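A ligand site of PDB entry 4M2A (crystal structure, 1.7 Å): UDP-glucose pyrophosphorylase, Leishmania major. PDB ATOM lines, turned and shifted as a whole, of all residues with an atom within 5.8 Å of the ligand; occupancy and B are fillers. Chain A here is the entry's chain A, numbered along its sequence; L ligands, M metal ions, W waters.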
ATOM      1  N   LEU A  81      -1.669   4.190   7.939  1.00  0.00           N
ATOM      2  CA  LEU A  81      -0.533   4.482   7.111  1.00  0.00           C
ATOM      3  C   LEU A  81      -0.458   5.974   6.754  1.00  0.00           C
ATOM      4  O   LEU A  81      -1.425   6.580   6.515  1.00  0.00           O
ATOM      5  CB  LEU A  81      -0.641   3.648   5.876  1.00  0.00           C
ATOM      6  CG  LEU A  81      -0.647   2.158   6.008  1.00  0.00           C
ATOM      7  CD1 LEU A  81      -0.890   1.447   4.705  1.00  0.00           C
ATOM      8  CD2 LEU A  81       0.592   1.603   6.651  1.00  0.00           C
ATOM      9  N   ASN A  82       0.747   6.546   6.778  1.00  0.00           N
ATOM     10  CA  ASN A  82       0.849   7.959   6.582  1.00  0.00           C
ATOM     11  C   ASN A  82       2.208   8.313   6.040  1.00  0.00           C
ATOM     12  O   ASN A  82       2.645   9.374   6.314  1.00  0.00           O
ATOM     13  CB  ASN A  82       0.646   8.636   7.902  1.00  0.00           C
ATOM     14  CG  ASN A  82       0.394  10.118   7.808  1.00  0.00           C
ATOM     15  OD1 ASN A  82      -0.296  10.569   6.973  1.00  0.00           O
ATOM     16  ND2 ASN A  82       0.936  10.836   8.725  1.00  0.00           N
ATOM     17  N   GLY A  83       2.870   7.363   5.399  1.00  0.00           N
ATOM     18  CA  GLY A  83       4.196   7.556   4.883  1.00  0.00           C
ATOM     19  C   GLY A  83       4.428   7.984   3.446  1.00  0.00           C
ATOM     20  O   GLY A  83       5.525   8.342   3.093  1.00  0.00           O
ATOM     21  N   GLY A  84       3.403   7.932   2.637  1.00  0.00           N
ATOM     22  CA  GLY A  84       3.545   8.321   1.240  1.00  0.00           C
ATOM     23  C   GLY A  84       3.454   9.810   0.917  1.00  0.00           C
ATOM     24  O   GLY A  84       3.318  10.641   1.788  1.00  0.00           O
ATOM     25  N   LEU A  85       3.412  10.129  -0.367  1.00  0.00           N
ATOM     26  CA  LEU A  85       3.678  11.497  -0.872  1.00  0.00           C
ATOM     27  C   LEU A  85       2.556  12.132  -1.671  1.00  0.00           C
ATOM     28  O   LEU A  85       2.573  13.350  -1.912  1.00  0.00           O
ATOM     29  CB  LEU A  85       4.896  11.449  -1.758  1.00  0.00           C
ATOM     30  CG  LEU A  85       6.205  11.439  -1.000  1.00  0.00           C
ATOM     31  CD1 LEU A  85       7.091  10.366  -1.601  1.00  0.00           C
ATOM     32  CD2 LEU A  85       6.797  12.838  -1.089  1.00  0.00           C
ATOM     33  N   LYS A  95      -0.621  13.717   2.704  1.00  0.00           N
ATOM     34  CA  LYS A  95      -1.947  13.839   2.108  1.00  0.00           C
ATOM     35  C   LYS A  95      -2.965  14.015   3.174  1.00  0.00           C
ATOM     36  O   LYS A  95      -3.952  14.671   2.956  1.00  0.00           O
ATOM     37  CB  LYS A  95      -2.257  12.552   1.349  1.00  0.00           C
ATOM     38  CG  LYS A  95      -3.621  12.630   0.671  1.00  0.00           C
ATOM     39  CD  LYS A  95      -3.895  11.366  -0.085  1.00  0.00           C
ATOM     40  CE  LYS A  95      -3.152  11.242  -1.344  1.00  0.00           C
ATOM     41  NZ  LYS A  95      -3.440   9.965  -2.044  1.00  0.00           N
ATOM     42  N   MET A 130       2.041   5.230  10.787  1.00  0.00           N
ATOM     43  CA  MET A 130       3.351   4.956  10.202  1.00  0.00           C
ATOM     44  C   MET A 130       3.746   6.175   9.347  1.00  0.00           C
ATOM     45  O   MET A 130       3.061   6.496   8.360  1.00  0.00           O
ATOM     46  CB  MET A 130       3.328   3.637   9.361  1.00  0.00           C
ATOM     47  CG  MET A 130       4.731   3.451   8.807  1.00  0.00           C
ATOM     48  SD  MET A 130       4.869   1.853   7.999  1.00  0.00           S
ATOM     49  CE  MET A 130       4.388   2.231   6.301  1.00  0.00           C
ATOM     50  N   GLN A 162       8.815   4.581   9.138  1.00  0.00           N
ATOM     51  CA  GLN A 162       9.195   3.623   8.113  1.00  0.00           C
ATOM     52  C   GLN A 162      10.683   3.771   7.756  1.00  0.00           C
ATOM     53  O   GLN A 162      11.324   4.807   8.052  1.00  0.00           O
ATOM     54  CB  GLN A 162       8.298   3.762   6.882  1.00  0.00           C
ATOM     55  CG  GLN A 162       8.485   5.059   6.144  1.00  0.00           C
ATOM     56  CD  GLN A 162       7.533   5.169   4.887  1.00  0.00           C
ATOM     57  OE1 GLN A 162       6.421   4.671   4.898  1.00  0.00           O
ATOM     58  NE2 GLN A 162       8.017   5.872   3.848  1.00  0.00           N
ATOM     59  N   PRO A 188      11.407   5.516   0.202  1.00  0.00           N
ATOM     60  CA  PRO A 188      10.646   4.744   1.141  1.00  0.00           C
ATOM     61  C   PRO A 188      10.308   3.391   0.432  1.00  0.00           C
ATOM     62  O   PRO A 188      10.267   3.324  -0.813  1.00  0.00           O
ATOM     63  CB  PRO A 188       9.410   5.639   1.377  1.00  0.00           C
ATOM     64  CG  PRO A 188       9.162   6.214   0.029  1.00  0.00           C
ATOM     65  CD  PRO A 188      10.540   6.395  -0.633  1.00  0.00           C
ATOM     66  N   PRO A 189      10.285   2.271   1.182  1.00  0.00           N
ATOM     67  CA  PRO A 189      10.178   0.971   0.514  1.00  0.00           C
ATOM     68  C   PRO A 189       8.739   0.460   0.355  1.00  0.00           C
ATOM     69  O   PRO A 189       8.558  -0.732   0.285  1.00  0.00           O
ATOM     70  CB  PRO A 189      10.946   0.010   1.445  1.00  0.00           C
ATOM     71  CG  PRO A 189      11.040   0.706   2.711  1.00  0.00           C
ATOM     72  CD  PRO A 189      10.490   2.089   2.622  1.00  0.00           C
ATOM     73  N   GLY A 190       7.792   1.375   0.304  1.00  0.00           N
ATOM     74  CA  GLY A 190       6.404   1.003   0.148  1.00  0.00           C
ATOM     75  C   GLY A 190       5.792   0.676   1.507  1.00  0.00           C
ATOM     76  O   GLY A 190       6.455   0.513   2.508  1.00  0.00           O
ATOM     77  N   HIS A 191       4.467   0.630   1.549  1.00  0.00           N
ATOM     78  CA  HIS A 191       3.884   0.390   2.877  1.00  0.00           C
ATOM     79  C   HIS A 191       4.070  -1.024   3.345  1.00  0.00           C
ATOM     80  O   HIS A 191       3.738  -1.342   4.510  1.00  0.00           O
ATOM     81  CB  HIS A 191       2.372   0.792   2.859  1.00  0.00           C
ATOM     82  CG  HIS A 191       1.624   0.352   1.642  1.00  0.00           C
ATOM     83  ND1 HIS A 191       1.362  -0.919   1.388  1.00  0.00           N
ATOM     84  CD2 HIS A 191       1.039   1.092   0.632  1.00  0.00           C
ATOM     85  CE1 HIS A 191       0.695  -1.021   0.172  1.00  0.00           C
ATOM     86  NE2 HIS A 191       0.493   0.207  -0.276  1.00  0.00           N
ATOM     87  N   SER A 218      -5.088   0.575   8.069  1.00  0.00           N
ATOM     88  CA  SER A 218      -5.758   1.046   6.856  1.00  0.00           C
ATOM     89  C   SER A 218      -4.995   2.215   6.262  1.00  0.00           C
ATOM     90  O   SER A 218      -4.137   2.819   6.994  1.00  0.00           O
ATOM     91  CB  SER A 218      -7.243   1.410   7.177  1.00  0.00           C
ATOM     92  OG  SER A 218      -7.278   2.440   8.137  1.00  0.00           O
ATOM     93  N   ASN A 219      -5.411   2.652   5.044  1.00  0.00           N
ATOM     94  CA  ASN A 219      -4.703   3.777   4.369  1.00  0.00           C
ATOM     95  C   ASN A 219      -5.108   5.091   5.013  1.00  0.00           C
ATOM     96  O   ASN A 219      -6.279   5.247   5.499  1.00  0.00           O
ATOM     97  CB  ASN A 219      -5.133   3.857   2.920  1.00  0.00           C
ATOM     98  CG  ASN A 219      -4.596   2.716   2.114  1.00  0.00           C
ATOM     99  OD1 ASN A 219      -3.567   2.100   2.479  1.00  0.00           O
ATOM    100  ND2 ASN A 219      -5.253   2.413   1.022  1.00  0.00           N
ATOM    101  N   GLY A 220      -4.137   5.953   5.174  1.00  0.00           N
ATOM    102  CA  GLY A 220      -4.426   7.322   5.727  1.00  0.00           C
ATOM    103  C   GLY A 220      -5.493   8.018   4.859  1.00  0.00           C
ATOM    104  O   GLY A 220      -6.169   8.847   5.381  1.00  0.00           O
ATOM    105  N   ASP A 221      -5.658   7.670   3.572  1.00  0.00           N
ATOM    106  CA  ASP A 221      -6.623   8.405   2.743  1.00  0.00           C
ATOM    107  C   ASP A 221      -7.997   7.801   2.782  1.00  0.00           C
ATOM    108  O   ASP A 221      -8.923   8.347   2.223  1.00  0.00           O
ATOM    109  CB  ASP A 221      -6.164   8.476   1.328  1.00  0.00           C
ATOM    110  CG  ASP A 221      -6.013   7.101   0.717  1.00  0.00           C
ATOM    111  OD1 ASP A 221      -4.954   6.488   0.882  1.00  0.00           O
ATOM    112  OD2 ASP A 221      -6.935   6.623   0.067  1.00  0.00           O
ATOM    113  N   LYS A 255      -6.445   2.420  -9.409  1.00  0.00           N
ATOM    114  CA  LYS A 255      -5.144   2.603  -8.746  1.00  0.00           C
ATOM    115  C   LYS A 255      -5.118   1.845  -7.407  1.00  0.00           C
ATOM    116  O   LYS A 255      -5.661   2.311  -6.389  1.00  0.00           O
ATOM    117  CB  LYS A 255      -4.813   4.085  -8.523  1.00  0.00           C
ATOM    118  CG  LYS A 255      -4.682   4.915  -9.811  1.00  0.00           C
ATOM    119  CD  LYS A 255      -4.519   6.417  -9.468  1.00  0.00           C
ATOM    120  CE  LYS A 255      -4.149   7.286 -10.683  1.00  0.00           C
ATOM    121  NZ  LYS A 255      -2.938   6.835 -11.410  1.00  0.00           N
ATOM    122  N   GLY A 256      -4.478   0.692  -7.462  1.00  0.00           N
ATOM    123  CA  GLY A 256      -4.448  -0.217  -6.294  1.00  0.00           C
ATOM    124  C   GLY A 256      -4.232  -1.631  -6.723  1.00  0.00           C
ATOM    125  O   GLY A 256      -3.472  -1.871  -7.662  1.00  0.00           O
ATOM    126  N   GLY A 257      -4.834  -2.598  -6.029  1.00  0.00           N
ATOM    127  CA  GLY A 257      -4.542  -4.009  -6.316  1.00  0.00           C
ATOM    128  C   GLY A 257      -5.805  -4.789  -6.111  1.00  0.00           C
ATOM    129  O   GLY A 257      -6.699  -4.340  -5.409  1.00  0.00           O
ATOM    130  N   HIS A 258      -5.812  -5.952  -6.758  1.00  0.00           N
ATOM    131  CA  HIS A 258      -6.906  -6.906  -6.619  1.00  0.00           C
ATOM    132  C   HIS A 258      -6.433  -8.213  -6.020  1.00  0.00           C
ATOM    133  O   HIS A 258      -5.274  -8.629  -6.067  1.00  0.00           O
ATOM    134  CB  HIS A 258      -7.627  -7.122  -7.955  1.00  0.00           C
ATOM    135  CG  HIS A 258      -6.785  -7.871  -8.953  1.00  0.00           C
ATOM    136  ND1 HIS A 258      -6.587  -9.175  -8.882  1.00  0.00           N
ATOM    137  CD2 HIS A 258      -6.010  -7.411 -10.011  1.00  0.00           C
ATOM    138  CE1 HIS A 258      -5.801  -9.569  -9.870  1.00  0.00           C
ATOM    139  NE2 HIS A 258      -5.443  -8.486 -10.552  1.00  0.00           N
ATOM    140  N   LEU A 282      -2.065 -10.834  -3.618  1.00  0.00           N
ATOM    141  CA  LEU A 282      -2.421  -9.522  -4.063  1.00  0.00           C
ATOM    142  C   LEU A 282      -1.706  -9.242  -5.347  1.00  0.00           C
ATOM    143  O   LEU A 282      -0.545  -9.639  -5.433  1.00  0.00           O
ATOM    144  CB  LEU A 282      -1.978  -8.541  -2.968  1.00  0.00           C
ATOM    145  CG  LEU A 282      -2.164  -7.102  -3.371  1.00  0.00           C
ATOM    146  CD1 LEU A 282      -3.664  -6.764  -3.436  1.00  0.00           C
ATOM    147  CD2 LEU A 282      -1.445  -6.183  -2.356  1.00  0.00           C
ATOM    148  N   GLU A 284      -0.902  -5.874  -7.348  1.00  0.00           N
ATOM    149  CA  GLU A 284      -0.965  -4.421  -7.536  1.00  0.00           C
ATOM    150  C   GLU A 284      -0.907  -4.064  -9.023  1.00  0.00           C
ATOM    151  O   GLU A 284      -0.370  -4.867  -9.828  1.00  0.00           O
ATOM    152  CB  GLU A 284       0.290  -3.815  -6.914  1.00  0.00           C
ATOM    153  CG  GLU A 284       0.328  -4.009  -5.392  1.00  0.00           C
ATOM    154  CD  GLU A 284      -0.737  -3.192  -4.742  1.00  0.00           C
ATOM    155  OE1 GLU A 284      -0.532  -1.946  -4.396  1.00  0.00           O
ATOM    156  OE2 GLU A 284      -1.889  -3.745  -4.487  1.00  0.00           O
ATOM    157  N   PHE A 305     -11.378  -5.942  -4.954  1.00  0.00           N
ATOM    158  CA  PHE A 305     -10.356  -4.909  -4.944  1.00  0.00           C
ATOM    159  C   PHE A 305      -9.928  -4.769  -3.474  1.00  0.00           C
ATOM    160  O   PHE A 305     -10.747  -4.713  -2.542  1.00  0.00           O
ATOM    161  CB  PHE A 305     -10.961  -3.632  -5.445  1.00  0.00           C
ATOM    162  CG  PHE A 305      -9.939  -2.605  -5.854  1.00  0.00           C
ATOM    163  CD1 PHE A 305      -9.194  -2.833  -6.986  1.00  0.00           C
ATOM    164  CD2 PHE A 305      -9.732  -1.426  -5.115  1.00  0.00           C
ATOM    165  CE1 PHE A 305      -8.290  -1.895  -7.453  1.00  0.00           C
ATOM    166  CE2 PHE A 305      -8.785  -0.488  -5.555  1.00  0.00           C
ATOM    167  CZ  PHE A 305      -8.072  -0.738  -6.713  1.00  0.00           C
ATOM    168  N   ASN A 306      -8.610  -4.815  -3.289  1.00  0.00           N
ATOM    169  CA  ASN A 306      -8.106  -4.628  -1.908  1.00  0.00           C
ATOM    170  C   ASN A 306      -8.414  -3.240  -1.443  1.00  0.00           C
ATOM    171  O   ASN A 306      -8.031  -2.238  -2.074  1.00  0.00           O
ATOM    172  CB  ASN A 306      -6.599  -4.874  -1.936  1.00  0.00           C
ATOM    173  CG  ASN A 306      -5.955  -4.728  -0.590  1.00  0.00           C
ATOM    174  OD1 ASN A 306      -6.621  -4.967   0.422  1.00  0.00           O
ATOM    175  ND2 ASN A 306      -4.697  -4.289  -0.568  1.00  0.00           N
ATOM    176  N   THR A 307      -9.002  -3.177  -0.240  1.00  0.00           N
ATOM    177  CA  THR A 307      -9.210  -1.880   0.406  1.00  0.00           C
ATOM    178  C   THR A 307      -7.977  -1.401   1.100  1.00  0.00           C
ATOM    179  O   THR A 307      -7.916  -0.185   1.463  1.00  0.00           O
ATOM    180  CB  THR A 307     -10.310  -1.957   1.507  1.00  0.00           C
ATOM    181  OG1 THR A 307      -9.923  -2.872   2.508  1.00  0.00           O
ATOM    182  CG2 THR A 307     -11.685  -2.406   0.913  1.00  0.00           C
ATOM    183  N   ASN A 308      -7.078  -2.333   1.428  1.00  0.00           N
ATOM    184  CA  ASN A 308      -5.937  -2.117   2.309  1.00  0.00           C
ATOM    185  C   ASN A 308      -6.349  -1.908   3.756  1.00  0.00           C
ATOM    186  O   ASN A 308      -5.536  -1.437   4.559  1.00  0.00           O
ATOM    187  CB  ASN A 308      -5.005  -0.974   1.813  1.00  0.00           C
ATOM    188  CG  ASN A 308      -3.540  -1.416   1.766  1.00  0.00           C
ATOM    189  OD1 ASN A 308      -3.251  -2.552   1.675  1.00  0.00           O
ATOM    190  ND2 ASN A 308      -2.609  -0.476   1.832  1.00  0.00           N
ATOM    191  N   ALA A 355       4.114  -4.222  -0.950  1.00  0.00           N
ATOM    192  CA  ALA A 355       2.764  -3.784  -0.568  1.00  0.00           C
ATOM    193  C   ALA A 355       2.275  -4.588   0.665  1.00  0.00           C
ATOM    194  O   ALA A 355       2.447  -5.777   0.723  1.00  0.00           O
ATOM    195  CB  ALA A 355       1.855  -4.074  -1.756  1.00  0.00           C
ATOM    196  N   MET A 356       1.806  -3.857   1.689  1.00  0.00           N
ATOM    197  CA  MET A 356       1.414  -4.601   2.879  1.00  0.00           C
ATOM    198  C   MET A 356       0.315  -5.632   2.713  1.00  0.00           C
ATOM    199  O   MET A 356       0.307  -6.648   3.467  1.00  0.00           O
ATOM    200  CB  MET A 356       1.097  -3.657   4.042  1.00  0.00           C
ATOM    201  CG  MET A 356      -0.191  -2.864   3.831  1.00  0.00           C
ATOM    202  SD  MET A 356      -0.700  -2.239   5.474  1.00  0.00           S
ATOM    203  CE  MET A 356      -2.368  -1.780   5.020  1.00  0.00           C
ATOM    204  N   GLY A 357      -0.544  -5.480   1.717  1.00  0.00           N
ATOM    205  CA  GLY A 357      -1.545  -6.481   1.529  1.00  0.00           C
ATOM    206  C   GLY A 357      -1.006  -7.789   0.966  1.00  0.00           C
ATOM    207  O   GLY A 357      -1.647  -8.800   0.998  1.00  0.00           O
ATOM    208  N   PHE A 376     -14.631   1.834   2.469  1.00  0.00           N
ATOM    209  CA  PHE A 376     -13.627   2.113   1.457  1.00  0.00           C
ATOM    210  C   PHE A 376     -13.948   3.398   0.680  1.00  0.00           C
ATOM    211  O   PHE A 376     -14.771   3.373  -0.292  1.00  0.00           O
ATOM    212  CB  PHE A 376     -13.504   0.921   0.500  1.00  0.00           C
ATOM    213  CG  PHE A 376     -12.380   1.083  -0.478  1.00  0.00           C
ATOM    214  CD1 PHE A 376     -11.098   1.295  -0.005  1.00  0.00           C
ATOM    215  CD2 PHE A 376     -12.593   0.867  -1.845  1.00  0.00           C
ATOM    216  CE1 PHE A 376     -10.044   1.434  -0.910  1.00  0.00           C
ATOM    217  CE2 PHE A 376     -11.557   1.042  -2.784  1.00  0.00           C
ATOM    218  CZ  PHE A 376     -10.269   1.271  -2.299  1.00  0.00           C
ATOM    219  N   PRO A 378     -11.482   5.667  -0.954  1.00  0.00           N
ATOM    220  CA  PRO A 378     -10.053   5.982  -1.263  1.00  0.00           C
ATOM    221  C   PRO A 378      -9.953   7.366  -1.825  1.00  0.00           C
ATOM    222  O   PRO A 378     -10.834   7.840  -2.589  1.00  0.00           O
ATOM    223  CB  PRO A 378      -9.672   4.913  -2.375  1.00  0.00           C
ATOM    224  CG  PRO A 378     -10.996   4.589  -2.963  1.00  0.00           C
ATOM    225  CD  PRO A 378     -11.945   4.548  -1.805  1.00  0.00           C
ATOM    226  N   VAL A 379      -8.855   8.046  -1.524  1.00  0.00           N
ATOM    227  CA  VAL A 379      -8.557   9.315  -2.174  1.00  0.00           C
ATOM    228  C   VAL A 379      -7.147   9.190  -2.802  1.00  0.00           C
ATOM    229  O   VAL A 379      -6.112   9.352  -2.066  1.00  0.00           O
ATOM    230  CB  VAL A 379      -8.610  10.532  -1.231  1.00  0.00           C
ATOM    231  CG1 VAL A 379      -8.203  11.781  -2.026  1.00  0.00           C
ATOM    232  CG2 VAL A 379      -9.963  10.762  -0.646  1.00  0.00           C
ATOM    233  N   LYS A 380      -7.063   8.823  -4.090  1.00  0.00           N
ATOM    234  CA  LYS A 380      -5.765   8.635  -4.791  1.00  0.00           C
ATOM    235  C   LYS A 380      -5.549   9.783  -5.746  1.00  0.00           C
ATOM    236  O   LYS A 380      -4.410  10.073  -6.186  1.00  0.00           O
ATOM    237  CB  LYS A 380      -5.753   7.355  -5.646  1.00  0.00           C
ATOM    238  CG  LYS A 380      -6.049   6.021  -4.939  1.00  0.00           C
ATOM    239  CD  LYS A 380      -5.073   5.778  -3.763  1.00  0.00           C
ATOM    240  CE  LYS A 380      -5.755   4.997  -2.641  1.00  0.00           C
ATOM    241  NZ  LYS A 380      -4.892   4.746  -1.422  1.00  0.00           N
HETATM  242  N1  LIG L   1       2.345   4.756   2.253  1.00  0.00           N
HETATM  243  C1  LIG L   1       3.335   4.638   3.270  1.00  0.00           C
HETATM  244  N2  LIG L   1       4.583   4.423   2.895  1.00  0.00           N
HETATM  245  C2  LIG L   1       4.861   4.135   1.605  1.00  0.00           C
HETATM  246  C3  LIG L   1       3.874   4.200   0.581  1.00  0.00           C
HETATM  247  C4  LIG L   1       2.576   4.463   0.973  1.00  0.00           C
HETATM  248  O1  LIG L   1       3.012   4.864   4.466  1.00  0.00           O
HETATM  249  O2  LIG L   1       6.084   3.888   1.297  1.00  0.00           O
HETATM  250  C5  LIG L   1       0.970   4.994   2.628  1.00  0.00           C
HETATM  251  C6  LIG L   1       0.228   6.090   1.892  1.00  0.00           C
HETATM  252  O3  LIG L   1       0.557   7.360   2.462  1.00  0.00           O
HETATM  253  C7  LIG L   1      -1.229   5.704   2.023  1.00  0.00           C
HETATM  254  C8  LIG L   1      -1.140   4.196   1.990  1.00  0.00           C
HETATM  255  O4  LIG L   1       0.238   3.796   2.275  1.00  0.00           O
HETATM  256  O5  LIG L   1      -1.646   6.084   3.347  1.00  0.00           O
HETATM  257  C9  LIG L   1      -1.460   3.486   0.663  1.00  0.00           C
HETATM  258  O6  LIG L   1      -0.572   4.081  -0.353  1.00  0.00           O
HETATM  259  P1  LIG L   1      -1.256   4.575  -1.749  1.00  0.00           P
HETATM  260  O7  LIG L   1      -2.281   5.592  -1.541  1.00  0.00           O
HETATM  261  O8  LIG L   1      -0.043   4.855  -2.696  1.00  0.00           O
HETATM  262  O9  LIG L   1      -1.925   3.258  -2.344  1.00  0.00           O
HETATM  263  P2  LIG L   1      -1.403   2.055  -3.164  1.00  0.00           P
HETATM  264  O10 LIG L   1      -0.206   1.570  -2.507  1.00  0.00           O
HETATM  265  O11 LIG L   1      -1.373   2.403  -4.629  1.00  0.00           O
HETATM  266  O12 LIG L   1      -2.637   1.055  -3.012  1.00  0.00           O
HETATM  267  C10 LIG L   1      -2.920   0.473  -1.766  1.00  0.00           C
HETATM  268  C11 LIG L   1      -2.864  -1.049  -1.851  1.00  0.00           C
HETATM  269  C12 LIG L   1      -3.827  -1.596  -2.963  1.00  0.00           C
HETATM  270  C13 LIG L   1      -5.200  -1.068  -2.549  1.00  0.00           C
HETATM  271  C14 LIG L   1      -5.243   0.465  -2.446  1.00  0.00           C
HETATM  272  C15 LIG L   1      -6.636   0.832  -1.926  1.00  0.00           C
HETATM  273  O13 LIG L   1      -1.495  -1.471  -1.938  1.00  0.00           O
HETATM  274  O14 LIG L   1      -3.765  -2.972  -2.894  1.00  0.00           O
HETATM  275  O15 LIG L   1      -6.116  -1.407  -3.595  1.00  0.00           O
HETATM  276  O16 LIG L   1      -4.245   0.873  -1.490  1.00  0.00           O
HETATM  277  O17 LIG L   1      -6.761   2.249  -2.009  1.00  0.00           O
HETATM  278 MG    MG M   1       1.642   6.789  -1.422  1.00  0.00          MG
HETATM  279  O   HOH W   1      -1.987   7.890  -3.293  1.00  0.00           O
HETATM  280  O   HOH W   2       0.653   5.699  -5.150  1.00  0.00           O
HETATM  281  O   HOH W   3      -2.367   8.795   3.088  1.00  0.00           O
HETATM  282  O   HOH W   4       2.343   3.147  -2.137  1.00  0.00           O
HETATM  283  O   HOH W   5      -2.673   8.003  -0.143  1.00  0.00           O
HETATM  284  O   HOH W   6       1.746  -0.658  -3.891  1.00  0.00           O
HETATM  285  O   HOH W   7      -7.620   3.906   0.295  1.00  0.00           O
HETATM  286  O   HOH W   8      -1.404  -3.566  -0.095  1.00  0.00           O
HETATM  287  O   HOH W   9      -2.764   4.132  -5.915  1.00  0.00           O
HETATM  288  O   HOH W  10       1.013   3.395  -6.055  1.00  0.00           O
HETATM  289  O   HOH W  11       6.781   4.566  -1.566  1.00  0.00           O
HETATM  290  O   HOH W  12      -1.119   0.040  -6.231  1.00  0.00           O
HETATM  291  O   HOH W  13      -7.645   2.745  -4.489  1.00  0.00           O
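N of Asn 306 sits at hydrogen-bond distance from O of Gly 257, 2.9 Å away. The backbone NH (N) of Gly 83 is in hydrogen-bond range of the backbone carbonyl oxygen (O) of Met 130, 3.1 Å away. A ring nitrogen (ND1) of His 191 is in hydrogen-bond range of the backbone NH (N) of Met 356. The side-chain amide nitrogen of Asn 219 lies close to the side-chain amino group of Lys 380, at 3.4 Å. NZ of Lys 380 lies within salt-bridge range of OD1 of Asp 221 (2.9 Å). The backbone NH (N) of Gly 220 sits at hydrogen-bond distance from the backbone carbonyl oxygen (O) of Leu 81, 3.1 Å away. The backbone carbonyl oxygen of Met 130 sits at hydrogen-bond distance from the backbone NH of Asn 82 (2.8 Å). N of Val 379 sits at hydrogen-bond distance from OD2 of Asp 221.
Water W9 bridges an oxygen (O11) of the ligand (2.6 Å) and the backbone carbonyl oxygen (O) of Lys 255 (3.5 Å). Water W13 lies within hydrogen-bond range of an oxygen (O17) of the ligand and the backbone carbonyl oxygen of Lys 255. Water W8 lies within hydrogen-bond range of OD1 of Asn 308, N of Gly 357, O13 of the ligand and ND2 of Asn 306. Water W12 lies within hydrogen-bond range of OE1 of Glu 284 (2.8 Å), O11 of the ligand (2.9 Å) and O of Gly 256 (3.4 Å). Water W1 bridges the side-chain amino group (NZ) of Lys 95 and an oxygen (O7) of the ligand. Water W6 lies within hydrogen-bond range of OE1 of Glu 284 (2.7 Å) and O10 of the ligand (3.3 Å).
Residues that only touch the ligand: Asn 82 (3.6 Å), Met 130 (3.5 Å), Pro 188 (3.8 Å), Asp 221 (3.7 Å), Gly 256 (3.4 Å), Leu 282 (3.8 Å), Phe 305 (3.4 Å), Thr 307 (3.8 Å), Asn 308 (3.7 Å), Phe 376 (3.6 Å) and Pro 378 (3.96 Å). Hydrophobic or aromatic side chains within 4 Å of the ligand: Leu 81, Met 130, Pro 188, His 191, Leu 282, Phe 305, Phe 376 and Pro 378. 23 residues have an atom within 4 Å of the ligand: Leu 81, Asn 82, Gly 83, Gly 84, Met 130, Gln 162, Pro 188, Gly 190, His 191, Asn 219, Gly 220, Asp 221, Gly 256, Gly 257, Leu 282, Glu 284, Phe 305, Asn 306, Thr 307, Asn 308, Phe 376, Pro 378 and Lys 380. Along chain A the residues within 4 Å of the ligand span positions 81 to 380. The nearest printed residue that does not touch the ligand is Ala 355 (4.2 Å).
An oxygen (O14) of the ligand is in hydrogen-bond range of the side-chain carboxylate of Glu 284, at 2.6 Å. O of Asn 306 sits at hydrogen-bond distance from O15 of the ligand (2.6 Å). ND2 of Asn 306 lies within hydrogen-bond range of O14 of the ligand (2.8 Å). N of Gly 83 sits at hydrogen-bond distance from O1 of the ligand, 2.7 Å away. O10 of the ligand lies within hydrogen-bond range of NE2 of His 191 (2.7 Å). A nitrogen (N2) of the ligand lies within hydrogen-bond range of the side-chain amide oxygen (OE1) of Gln 162, at 2.7 Å. An oxygen (O7) of the ligand lies within salt-bridge range of the side-chain amino group of Lys 380. An oxygen (O3) of the ligand is in hydrogen-bond range of the backbone NH (N) of Gly 84 (2.9 Å). An oxygen (O15) of the ligand sits at hydrogen-bond distance from the backbone NH (N) of Gly 257 (3.0 Å). The backbone carbonyl oxygen (O) of Gly 257 lies within hydrogen-bond range of an oxygen (O15) of the ligand, at 3.5 Å. An oxygen (O5) of the ligand lies within hydrogen-bond range of the backbone NH of Gly 220, 3.1 Å away. The side-chain amide nitrogen of Asn 219 lies within hydrogen-bond range of an oxygen (O16) of the ligand, at 3.1 Å. The backbone NH of Gly 190 lies close to an oxygen (O2) of the ligand (3.2 Å). O of Leu 81 is in hydrogen-bond range of O5 of the ligand.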
